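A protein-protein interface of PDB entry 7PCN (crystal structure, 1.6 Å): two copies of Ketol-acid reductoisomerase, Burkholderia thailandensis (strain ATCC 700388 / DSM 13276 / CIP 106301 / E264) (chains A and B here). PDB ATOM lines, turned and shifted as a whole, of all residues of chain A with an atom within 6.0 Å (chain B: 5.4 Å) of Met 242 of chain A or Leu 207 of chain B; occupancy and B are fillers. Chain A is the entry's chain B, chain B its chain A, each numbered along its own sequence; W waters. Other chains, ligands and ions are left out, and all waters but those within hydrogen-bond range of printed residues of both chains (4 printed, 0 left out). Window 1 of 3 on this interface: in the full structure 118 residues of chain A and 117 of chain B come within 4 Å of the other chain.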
ATOM      1  N   LEU A 207      26.767  20.785  -8.630  1.00  0.00           N
ATOM      2  CA  LEU A 207      26.373  22.171  -8.280  1.00  0.00           C
ATOM      3  C   LEU A 207      27.153  22.625  -7.035  1.00  0.00           C
ATOM      4  O   LEU A 207      27.738  23.729  -7.051  1.00  0.00           O
ATOM      5  CB  LEU A 207      24.869  22.198  -8.030  1.00  0.00           C
ATOM      6  CG  LEU A 207      24.283  23.567  -7.714  1.00  0.00           C
ATOM      7  CD1 LEU A 207      22.812  23.604  -8.058  1.00  0.00           C
ATOM      8  CD2 LEU A 207      24.475  23.935  -6.251  1.00  0.00           C
ATOM      9  N   LEU A 210      30.799  23.049  -7.820  1.00  0.00           N
ATOM     10  CA  LEU A 210      31.038  24.278  -8.626  1.00  0.00           C
ATOM     11  C   LEU A 210      31.097  25.503  -7.702  1.00  0.00           C
ATOM     12  O   LEU A 210      32.031  26.309  -7.824  1.00  0.00           O
ATOM     13  CB  LEU A 210      29.913  24.417  -9.649  1.00  0.00           C
ATOM     14  CG  LEU A 210      30.017  25.628 -10.562  1.00  0.00           C
ATOM     15  CD1 LEU A 210      31.245  25.515 -11.455  1.00  0.00           C
ATOM     16  CD2 LEU A 210      28.752  25.748 -11.402  1.00  0.00           C
ATOM     17  N   VAL A 211      30.124  25.625  -6.804  1.00  0.00           N
ATOM     18  CA  VAL A 211      30.085  26.686  -5.758  1.00  0.00           C
ATOM     19  C   VAL A 211      31.393  26.633  -4.960  1.00  0.00           C
ATOM     20  O   VAL A 211      32.026  27.681  -4.765  1.00  0.00           O
ATOM     21  CB  VAL A 211      28.844  26.506  -4.872  1.00  0.00           C
ATOM     22  CG1 VAL A 211      28.919  27.329  -3.601  1.00  0.00           C
ATOM     23  CG2 VAL A 211      27.573  26.830  -5.645  1.00  0.00           C
ATOM     24  N   GLU A 237      22.052  35.213  -2.884  1.00  0.00           N
ATOM     25  CA  GLU A 237      21.799  35.767  -4.237  1.00  0.00           C
ATOM     26  C   GLU A 237      21.711  34.634  -5.265  1.00  0.00           C
ATOM     27  O   GLU A 237      20.770  34.643  -6.100  1.00  0.00           O
ATOM     28  CB  GLU A 237      22.868  36.760  -4.661  1.00  0.00           C
ATOM     29  CG  GLU A 237      22.488  37.502  -5.916  1.00  0.00           C
ATOM     30  CD  GLU A 237      23.463  38.600  -6.286  1.00  0.00           C
ATOM     31  OE1 GLU A 237      24.675  38.396  -6.069  1.00  0.00           O
ATOM     32  OE2 GLU A 237      23.014  39.645  -6.806  1.00  0.00           O
ATOM     33  N   MET A 238      22.659  33.707  -5.262  1.00  0.00           N
ATOM     34  CA  MET A 238      22.673  32.651  -6.310  1.00  0.00           C
ATOM     35  C   MET A 238      21.475  31.706  -6.100  1.00  0.00           C
ATOM     36  O   MET A 238      20.882  31.287  -7.095  1.00  0.00           O
ATOM     37  CB  MET A 238      24.002  31.897  -6.318  1.00  0.00           C
ATOM     38  CG  MET A 238      25.166  32.774  -6.775  1.00  0.00           C
ATOM     39  SD  MET A 238      24.914  33.624  -8.373  1.00  0.00           S
ATOM     40  CE  MET A 238      24.657  32.216  -9.452  1.00  0.00           C
ATOM     41  N   GLY A 239      21.065  31.449  -4.860  1.00  0.00           N
ATOM     42  CA  GLY A 239      19.841  30.676  -4.560  1.00  0.00           C
ATOM     43  C   GLY A 239      18.587  31.404  -5.027  1.00  0.00           C
ATOM     44  O   GLY A 239      17.693  30.746  -5.637  1.00  0.00           O
ATOM     45  N   LYS A 240      18.521  32.726  -4.822  1.00  0.00           N
ATOM     46  CA  LYS A 240      17.372  33.529  -5.318  1.00  0.00           C
ATOM     47  C   LYS A 240      17.322  33.429  -6.848  1.00  0.00           C
ATOM     48  O   LYS A 240      16.218  33.316  -7.400  1.00  0.00           O
ATOM     49  CB  LYS A 240      17.475  34.994  -4.892  1.00  0.00           C
ATOM     50  CG  LYS A 240      17.120  35.298  -3.444  1.00  0.00           C
ATOM     51  CD  LYS A 240      15.686  35.013  -3.039  1.00  0.00           C
ATOM     52  CE  LYS A 240      14.659  35.424  -4.067  1.00  0.00           C
ATOM     53  NZ  LYS A 240      13.307  35.517  -3.463  1.00  0.00           N
ATOM     54  N   MET A 241      18.478  33.480  -7.517  1.00  0.00           N
ATOM     55  CA  MET A 241      18.533  33.420  -8.996  1.00  0.00           C
ATOM     56  C   MET A 241      17.953  32.069  -9.452  1.00  0.00           C
ATOM     57  O   MET A 241      17.168  32.023 -10.420  1.00  0.00           O
ATOM     58  CB  MET A 241      19.966  33.579  -9.509  1.00  0.00           C
ATOM     59  CG  MET A 241      20.066  33.304 -10.992  1.00  0.00           C
ATOM     60  SD  MET A 241      21.624  33.867 -11.682  1.00  0.00           S
ATOM     61  CE  MET A 241      21.676  32.917 -13.200  1.00  0.00           C
ATOM     62  N   MET A 242      18.325  30.987  -8.777  1.00  0.00           N
ATOM     63  CA  MET A 242      17.875  29.622  -9.171  1.00  0.00           C
ATOM     64  C   MET A 242      16.378  29.445  -8.900  1.00  0.00           C
ATOM     65  O   MET A 242      15.695  28.780  -9.703  1.00  0.00           O
ATOM     66  CB  MET A 242      18.640  28.552  -8.406  1.00  0.00           C
ATOM     67  CG  MET A 242      20.069  28.434  -8.827  1.00  0.00           C
ATOM     68  SD  MET A 242      20.596  26.726  -8.658  1.00  0.00           S
ATOM     69  CE  MET A 242      19.640  26.083 -10.032  1.00  0.00           C
ATOM     70  N   LEU A 243      15.881  30.000  -7.799  1.00  0.00           N
ATOM     71  CA  LEU A 243      14.460  29.836  -7.416  1.00  0.00           C
ATOM     72  C   LEU A 243      13.597  30.758  -8.286  1.00  0.00           C
ATOM     73  O   LEU A 243      12.569  30.295  -8.798  1.00  0.00           O
ATOM     74  CB  LEU A 243      14.315  30.126  -5.925  1.00  0.00           C
ATOM     75  CG  LEU A 243      12.945  29.832  -5.321  1.00  0.00           C
ATOM     76  CD1 LEU A 243      12.532  28.383  -5.540  1.00  0.00           C
ATOM     77  CD2 LEU A 243      12.969  30.160  -3.838  1.00  0.00           C
ATOM     78  N   ASP A 244      14.023  31.998  -8.501  1.00  0.00           N
ATOM     79  CA  ASP A 244      13.336  32.914  -9.449  1.00  0.00           C
ATOM     80  C   ASP A 244      13.403  32.306 -10.858  1.00  0.00           C
ATOM     81  O   ASP A 244      12.400  32.412 -11.598  1.00  0.00           O
ATOM     82  CB  ASP A 244      13.927  34.325  -9.435  1.00  0.00           C
ATOM     83  CG  ASP A 244      13.660  35.140  -8.182  1.00  0.00           C
ATOM     84  OD1 ASP A 244      12.781  34.744  -7.395  1.00  0.00           O
ATOM     85  OD2 ASP A 244      14.326  36.192  -8.019  1.00  0.00           O
ATOM     86  N   GLY A 245      14.533  31.687 -11.216  1.00  0.00           N
ATOM     87  CA  GLY A 245      14.703  31.014 -12.516  1.00  0.00           C
ATOM     88  C   GLY A 245      13.647  29.933 -12.723  1.00  0.00           C
ATOM     89  O   GLY A 245      13.184  29.792 -13.869  1.00  0.00           O
ATOM     90  N   ALA A 246      13.253  29.196 -11.670  1.00  0.00           N
ATOM     91  CA  ALA A 246      12.165  28.192 -11.763  1.00  0.00           C
ATOM     92  C   ALA A 246      10.880  28.873 -12.253  1.00  0.00           C
ATOM     93  O   ALA A 246      10.141  28.253 -13.035  1.00  0.00           O
ATOM     94  CB  ALA A 246      11.952  27.479 -10.451  1.00  0.00           C
ATOM     95  N   ASP A 247      10.624  30.106 -11.831  1.00  0.00           N
ATOM     96  CA  ASP A 247       9.461  30.901 -12.306  1.00  0.00           C
ATOM     97  C   ASP A 247       9.693  31.356 -13.755  1.00  0.00           C
ATOM     98  O   ASP A 247       8.892  30.955 -14.626  1.00  0.00           O
ATOM     99  CB  ASP A 247       9.190  32.099 -11.393  1.00  0.00           C
ATOM    100  CG  ASP A 247       7.942  32.877 -11.762  1.00  0.00           C
ATOM    101  OD1 ASP A 247       7.108  32.333 -12.506  1.00  0.00           O
ATOM    102  OD2 ASP A 247       7.816  34.024 -11.292  1.00  0.00           O
ATOM    103  N   LEU A 250      16.200  30.889 -16.260  1.00  0.00           N
ATOM    104  CA  LEU A 250      17.496  31.276 -15.653  1.00  0.00           C
ATOM    105  C   LEU A 250      18.150  32.421 -16.436  1.00  0.00           C
ATOM    106  O   LEU A 250      18.595  33.382 -15.800  1.00  0.00           O
ATOM    107  CB  LEU A 250      18.385  30.041 -15.591  1.00  0.00           C
ATOM    108  CG  LEU A 250      17.963  29.038 -14.524  1.00  0.00           C
ATOM    109  CD1 LEU A 250      18.600  27.689 -14.771  1.00  0.00           C
ATOM    110  CD2 LEU A 250      18.288  29.553 -13.129  1.00  0.00           C
ATOM    111  N   VAL A 253      16.234  35.640 -15.668  1.00  0.00           N
ATOM    112  CA  VAL A 253      16.596  36.317 -14.388  1.00  0.00           C
ATOM    113  C   VAL A 253      17.726  37.305 -14.675  1.00  0.00           C
ATOM    114  O   VAL A 253      17.676  38.447 -14.203  1.00  0.00           O
ATOM    115  CB  VAL A 253      16.996  35.333 -13.277  1.00  0.00           C
ATOM    116  CG1 VAL A 253      17.560  36.083 -12.081  1.00  0.00           C
ATOM    117  CG2 VAL A 253      15.824  34.466 -12.859  1.00  0.00           C
ATOM    118  N   THR A 273      31.701  27.605 -20.236  1.00  0.00           N
ATOM    119  CA  THR A 273      32.435  27.484 -18.940  1.00  0.00           C
ATOM    120  C   THR A 273      32.894  26.046 -18.670  1.00  0.00           C
ATOM    121  O   THR A 273      33.886  25.879 -17.913  1.00  0.00           O
ATOM    122  CB  THR A 273      31.607  27.982 -17.754  1.00  0.00           C
ATOM    123  OG1 THR A 273      30.445  27.156 -17.637  1.00  0.00           O
ATOM    124  CG2 THR A 273      31.257  29.449 -17.904  1.00  0.00           C
ATOM    125  N   PHE B 202      32.245  33.741 -14.107  1.00  0.00           N
ATOM    126  CA  PHE B 202      32.529  32.306 -13.855  1.00  0.00           C
ATOM    127  C   PHE B 202      31.280  31.616 -13.293  1.00  0.00           C
ATOM    128  O   PHE B 202      30.709  30.742 -13.967  1.00  0.00           O
ATOM    129  CB  PHE B 202      33.730  32.091 -12.940  1.00  0.00           C
ATOM    130  CG  PHE B 202      33.869  30.633 -12.604  1.00  0.00           C
ATOM    131  CD1 PHE B 202      34.282  29.724 -13.565  1.00  0.00           C
ATOM    132  CD2 PHE B 202      33.471  30.156 -11.364  1.00  0.00           C
ATOM    133  CE1 PHE B 202      34.339  28.367 -13.272  1.00  0.00           C
ATOM    134  CE2 PHE B 202      33.554  28.805 -11.068  1.00  0.00           C
ATOM    135  CZ  PHE B 202      33.991  27.911 -12.021  1.00  0.00           C
ATOM    136  N   LEU B 203      30.844  32.010 -12.102  1.00  0.00           N
ATOM    137  CA  LEU B 203      29.912  31.173 -11.306  1.00  0.00           C
ATOM    138  C   LEU B 203      28.512  31.128 -11.932  1.00  0.00           C
ATOM    139  O   LEU B 203      27.987  30.006 -12.076  1.00  0.00           O
ATOM    140  CB  LEU B 203      29.825  31.658  -9.858  1.00  0.00           C
ATOM    141  CG  LEU B 203      28.904  30.782  -9.005  1.00  0.00           C
ATOM    142  CD1 LEU B 203      29.348  29.322  -9.029  1.00  0.00           C
ATOM    143  CD2 LEU B 203      28.824  31.279  -7.590  1.00  0.00           C
ATOM    144  N   ALA B 204      27.906  32.276 -12.257  1.00  0.00           N
ATOM    145  CA  ALA B 204      26.508  32.312 -12.738  1.00  0.00           C
ATOM    146  C   ALA B 204      26.408  31.534 -14.048  1.00  0.00           C
ATOM    147  O   ALA B 204      25.572  30.643 -14.171  1.00  0.00           O
ATOM    148  CB  ALA B 204      26.003  33.724 -12.855  1.00  0.00           C
ATOM    149  N   PRO B 205      27.249  31.796 -15.071  1.00  0.00           N
ATOM    150  CA  PRO B 205      27.156  31.014 -16.303  1.00  0.00           C
ATOM    151  C   PRO B 205      27.523  29.531 -16.135  1.00  0.00           C
ATOM    152  O   PRO B 205      26.948  28.696 -16.833  1.00  0.00           O
ATOM    153  CB  PRO B 205      28.130  31.666 -17.305  1.00  0.00           C
ATOM    154  CG  PRO B 205      28.775  32.821 -16.577  1.00  0.00           C
ATOM    155  CD  PRO B 205      28.188  32.918 -15.185  1.00  0.00           C
ATOM    156  N   ALA B 206      28.437  29.196 -15.226  1.00  0.00           N
ATOM    157  CA  ALA B 206      28.800  27.780 -14.998  1.00  0.00           C
ATOM    158  C   ALA B 206      27.610  27.039 -14.373  1.00  0.00           C
ATOM    159  O   ALA B 206      27.334  25.915 -14.787  1.00  0.00           O
ATOM    160  CB  ALA B 206      30.044  27.665 -14.168  1.00  0.00           C
ATOM    161  N   LEU B 207      26.907  27.665 -13.432  1.00  0.00           N
ATOM    162  CA  LEU B 207      25.723  27.069 -12.769  1.00  0.00           C
ATOM    163  C   LEU B 207      24.640  26.826 -13.822  1.00  0.00           C
ATOM    164  O   LEU B 207      24.071  25.718 -13.846  1.00  0.00           O
ATOM    165  CB  LEU B 207      25.276  28.032 -11.672  1.00  0.00           C
ATOM    166  CG  LEU B 207      24.107  27.626 -10.793  1.00  0.00           C
ATOM    167  CD1 LEU B 207      24.098  26.137 -10.486  1.00  0.00           C
ATOM    168  CD2 LEU B 207      24.168  28.428  -9.502  1.00  0.00           C
ATOM    169  N   VAL B 208      24.365  27.810 -14.680  1.00  0.00           N
ATOM    170  CA  VAL B 208      23.298  27.640 -15.707  1.00  0.00           C
ATOM    171  C   VAL B 208      23.784  26.627 -16.753  1.00  0.00           C
ATOM    172  O   VAL B 208      22.984  25.765 -17.153  1.00  0.00           O
ATOM    173  CB  VAL B 208      22.835  28.981 -16.305  1.00  0.00           C
ATOM    174  CG1 VAL B 208      21.715  28.762 -17.318  1.00  0.00           C
ATOM    175  CG2 VAL B 208      22.351  29.912 -15.206  1.00  0.00           C
ATOM    176  N   ASP B 209      25.060  26.661 -17.132  1.00  0.00           N
ATOM    177  CA  ASP B 209      25.627  25.670 -18.083  1.00  0.00           C
ATOM    178  C   ASP B 209      25.475  24.257 -17.501  1.00  0.00           C
ATOM    179  O   ASP B 209      25.171  23.329 -18.269  1.00  0.00           O
ATOM    180  CB  ASP B 209      27.095  25.942 -18.402  1.00  0.00           C
ATOM    181  CG  ASP B 209      27.353  27.144 -19.298  1.00  0.00           C
ATOM    182  OD1 ASP B 209      26.369  27.775 -19.778  1.00  0.00           O
ATOM    183  OD2 ASP B 209      28.538  27.422 -19.542  1.00  0.00           O
ATOM    184  N   LEU B 210      25.672  24.086 -16.196  1.00  0.00           N
ATOM    185  CA  LEU B 210      25.607  22.746 -15.556  1.00  0.00           C
ATOM    186  C   LEU B 210      24.156  22.258 -15.585  1.00  0.00           C
ATOM    187  O   LEU B 210      23.909  21.140 -16.002  1.00  0.00           O
ATOM    188  CB  LEU B 210      26.127  22.854 -14.123  1.00  0.00           C
ATOM    189  CG  LEU B 210      25.974  21.595 -13.277  1.00  0.00           C
ATOM    190  CD1 LEU B 210      26.811  20.452 -13.837  1.00  0.00           C
ATOM    191  CD2 LEU B 210      26.361  21.879 -11.836  1.00  0.00           C
ATOM    192  N   VAL B 211      23.227  23.094 -15.148  1.00  0.00           N
ATOM    193  CA  VAL B 211      21.771  22.780 -15.188  1.00  0.00           C
ATOM    194  C   VAL B 211      21.391  22.388 -16.619  1.00  0.00           C
ATOM    195  O   VAL B 211      20.664  21.393 -16.787  1.00  0.00           O
ATOM    196  CB  VAL B 211      20.961  23.976 -14.663  1.00  0.00           C
ATOM    197  CG1 VAL B 211      19.494  23.913 -15.025  1.00  0.00           C
ATOM    198  CG2 VAL B 211      21.127  24.112 -13.159  1.00  0.00           C
ATOM    199  N   GLU B 212      21.858  23.160 -17.603  1.00  0.00           N
ATOM    200  CA  GLU B 212      21.543  22.930 -19.031  1.00  0.00           C
ATOM    201  C   GLU B 212      22.148  21.598 -19.467  1.00  0.00           C
ATOM    202  O   GLU B 212      21.494  20.875 -20.231  1.00  0.00           O
ATOM    203  CB  GLU B 212      22.083  24.083 -19.876  1.00  0.00           C
ATOM    204  CG  GLU B 212      21.741  23.992 -21.343  1.00  0.00           C
ATOM    205  CD  GLU B 212      22.164  25.249 -22.078  1.00  0.00           C
ATOM    206  OE1 GLU B 212      23.386  25.484 -22.156  1.00  0.00           O
ATOM    207  OE2 GLU B 212      21.282  26.018 -22.519  1.00  0.00           O
ATOM    208  N   VAL B 232      16.113  19.533 -12.861  1.00  0.00           N
ATOM    209  CA  VAL B 232      17.394  20.296 -12.855  1.00  0.00           C
ATOM    210  C   VAL B 232      17.199  21.707 -12.274  1.00  0.00           C
ATOM    211  O   VAL B 232      18.179  22.226 -11.724  1.00  0.00           O
ATOM    212  CB  VAL B 232      18.111  20.283 -14.213  1.00  0.00           C
ATOM    213  CG1 VAL B 232      18.461  18.860 -14.631  1.00  0.00           C
ATOM    214  CG2 VAL B 232      17.328  20.990 -15.297  1.00  0.00           C
ATOM    215  N   TYR B 233      15.999  22.297 -12.338  1.00  0.00           N
ATOM    216  CA  TYR B 233      15.687  23.545 -11.597  1.00  0.00           C
ATOM    217  C   TYR B 233      14.185  23.841 -11.597  1.00  0.00           C
ATOM    218  O   TYR B 233      13.756  24.531 -10.680  1.00  0.00           O
ATOM    219  CB  TYR B 233      16.446  24.765 -12.149  1.00  0.00           C
ATOM    220  CG  TYR B 233      15.873  25.292 -13.441  1.00  0.00           C
ATOM    221  CD1 TYR B 233      16.168  24.685 -14.657  1.00  0.00           C
ATOM    222  CD2 TYR B 233      15.006  26.371 -13.448  1.00  0.00           C
ATOM    223  CE1 TYR B 233      15.604  25.133 -15.842  1.00  0.00           C
ATOM    224  CE2 TYR B 233      14.434  26.825 -14.625  1.00  0.00           C
ATOM    225  CZ  TYR B 233      14.726  26.201 -15.823  1.00  0.00           C
ATOM    226  OH  TYR B 233      14.155  26.664 -16.973  1.00  0.00           O
ATOM    227  N   MET B 238      16.019  22.555  -6.578  1.00  0.00           N
ATOM    228  CA  MET B 238      17.468  22.870  -6.528  1.00  0.00           C
ATOM    229  C   MET B 238      17.672  24.326  -6.055  1.00  0.00           C
ATOM    230  O   MET B 238      18.632  24.566  -5.274  1.00  0.00           O
ATOM    231  CB  MET B 238      18.148  22.612  -7.872  1.00  0.00           C
ATOM    232  CG  MET B 238      18.185  21.130  -8.244  1.00  0.00           C
ATOM    233  SD  MET B 238      18.856  20.053  -6.935  1.00  0.00           S
ATOM    234  CE  MET B 238      20.484  20.747  -6.656  1.00  0.00           C
ATOM    235  N   GLY B 239      16.806  25.269  -6.444  1.00  0.00           N
ATOM    236  CA  GLY B 239      16.872  26.652  -5.929  1.00  0.00           C
ATOM    237  C   GLY B 239      16.607  26.715  -4.432  1.00  0.00           C
ATOM    238  O   GLY B 239      17.315  27.460  -3.717  1.00  0.00           O
ATOM    239  N   MET B 242      19.747  25.637  -2.628  1.00  0.00           N
ATOM    240  CA  MET B 242      20.788  26.704  -2.613  1.00  0.00           C
ATOM    241  C   MET B 242      20.407  27.809  -1.619  1.00  0.00           C
ATOM    242  O   MET B 242      21.308  28.365  -0.960  1.00  0.00           O
ATOM    243  CB  MET B 242      20.945  27.320  -3.998  1.00  0.00           C
ATOM    244  CG  MET B 242      21.493  26.358  -4.987  1.00  0.00           C
ATOM    245  SD  MET B 242      22.281  27.256  -6.300  1.00  0.00           S
ATOM    246  CE  MET B 242      23.728  27.775  -5.371  1.00  0.00           C
HETATM  247  O   HOH W   1      22.175  30.905  -2.200  1.00  0.00           O
HETATM  248  O   HOH W   2      15.188  25.997  -8.779  1.00  0.00           O
HETATM  249  O   HOH W   3      16.066  28.500 -17.958  1.00  0.00           O
HETATM  250  O   HOH W   4      29.699  25.206 -20.837  1.00  0.00           O
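The side-chain carboxylate (OD2) of Asp 209 of chain B lies within hydrogen-bond range of the side-chain hydroxyl (OG1) of Thr 273 of chain A (2.7 Å).
The side-chain sulfur (SD) of Met 242 of chain A lies close to the side-chain sulfur (SD) of Met 242 of chain B.
Printed residues of chain B within 4 Å of Met 242 of chain A: Leu 207, Val 211, Gly 239 and Met 242.
Of the printed residues of chain A, Leu 207 of chain B touches Leu 207 (3.7 Å), Leu 210 (3.3 Å), Met 238 (3.8 Å) and Met 242 (3.99 Å).
Of the printed residues of chain B, Gly 245 of chain A touches Tyr 233.
Of the printed residues of chain B, Ala 246 of chain A touches Tyr 233.
Of the printed residues of chain B, Met 238 of chain A touches Ala 204 and Leu 207.
Lys 240 of chain A touches none of the printed residues of chain B.
The nearest printed residue of chain B that does not touch Met 242 of chain A is Tyr 233 of chain B (4.1 Å).
The nearest printed residue of chain A that does not touch Leu 207 of chain B is Val 211 of chain A (5.4 Å).
The nearest printed residue of chain A that does not touch Met 242 of chain B is Met 238 of chain A (4.2 Å).
Leu 207 of chain A touches its own counterpart, Leu 207 of chain B.
Leu 207 of chain A touches Met 238 of chain B, and with the chains exchanged Met 238 of chain A touches Leu 207 of chain B.
Val 211 of chain A touches Met 242 of chain B, and with the chains exchanged Met 242 of chain A touches Val 211 of chain B.
Met 242 of chain B touches its own counterpart, Met 242 of chain A.
6 positions are printed for both chains.
Of the 26 pairs that touch across the chains among the printed residues, 13 have their exchanged pair printed and touching as well.
Hydrophobic or aromatic side chains of chain A that line the printed part of chain B: Leu 207, Leu 210, Val 211, Met 238, Met 241, Met 242, Ala 246 and Leu 250.
Of the 16 printed residues of chain B, 13 touch a printed residue of chain A.
Among the printed residues, 26 pairs touch across the chains.
Among the printed residues, no Asp or Glu carboxylate lies within 4 Å of a Lys or Arg side-chain nitrogen of the other chain.
Among the printed residues, merely in contact across the chains: Thr 273 of chain A with Ala 206 of chain B, Gly 245 of chain A with Tyr 233 of chain B, Leu 210 of chain A with Leu 207 of chain B, Leu 207 of chain A with Leu 210 of chain B, Leu 210 of chain A with Ala 206 of chain B, Ala 246 of chain A with Tyr 233 of chain B, Gly 239 of chain A with Met 242 of chain B, Met 242 of chain A with Gly 239 of chain B, Met 241 of chain A with Val 208 of chain B, Leu 210 of chain A with Phe 202 of chain B, Leu 207 of chain A with Leu 207 of chain B, Met 238 of chain A with Ala 204 of chain B, Met 238 of chain A with Leu 207 of chain B, Gly 239 of chain A with Gly 239 of chain B, Leu 250 of chain A with Tyr 233 of chain B, Thr 273 of chain A with Pro 205 of chain B, Leu 250 of chain A with Val 211 of chain B, Leu 207 of chain A with Met 238 of chain B, Leu 243 of chain A with Gly 239 of chain B, Leu 250 of chain A with Val 208 of chain B, Val 211 of chain A with Met 242 of chain B, Leu 207 of chain A with Met 242 of chain B, Met 242 of chain A with Val 211 of chain B and Met 242 of chain A with Leu 207 of chain B.
Water W2 lies within hydrogen-bond range of the backbone carbonyl oxygen (O) of Tyr 233 of chain B (2.8 Å), the backbone NH (N) of Gly 239 of chain B (2.9 Å) and the backbone carbonyl oxygen (O) of Met 242 of chain A (3.0 Å).
Water W4 bridges the side-chain carboxylate (OD2) of Asp 209 of chain B (2.8 Å) and the backbone NH (N) of Thr 273 of chain A (3.2 Å).
Water W3 bridges the side-chain hydroxyl (OH) of Tyr 233 of chain B (2.8 Å) and the backbone NH (N) of Leu 250 of chain A (2.9 Å).
Water W1 bridges N of Gly 239 of chain A (2.9 Å) and O of Met 242 of chain B (3.0 Å).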
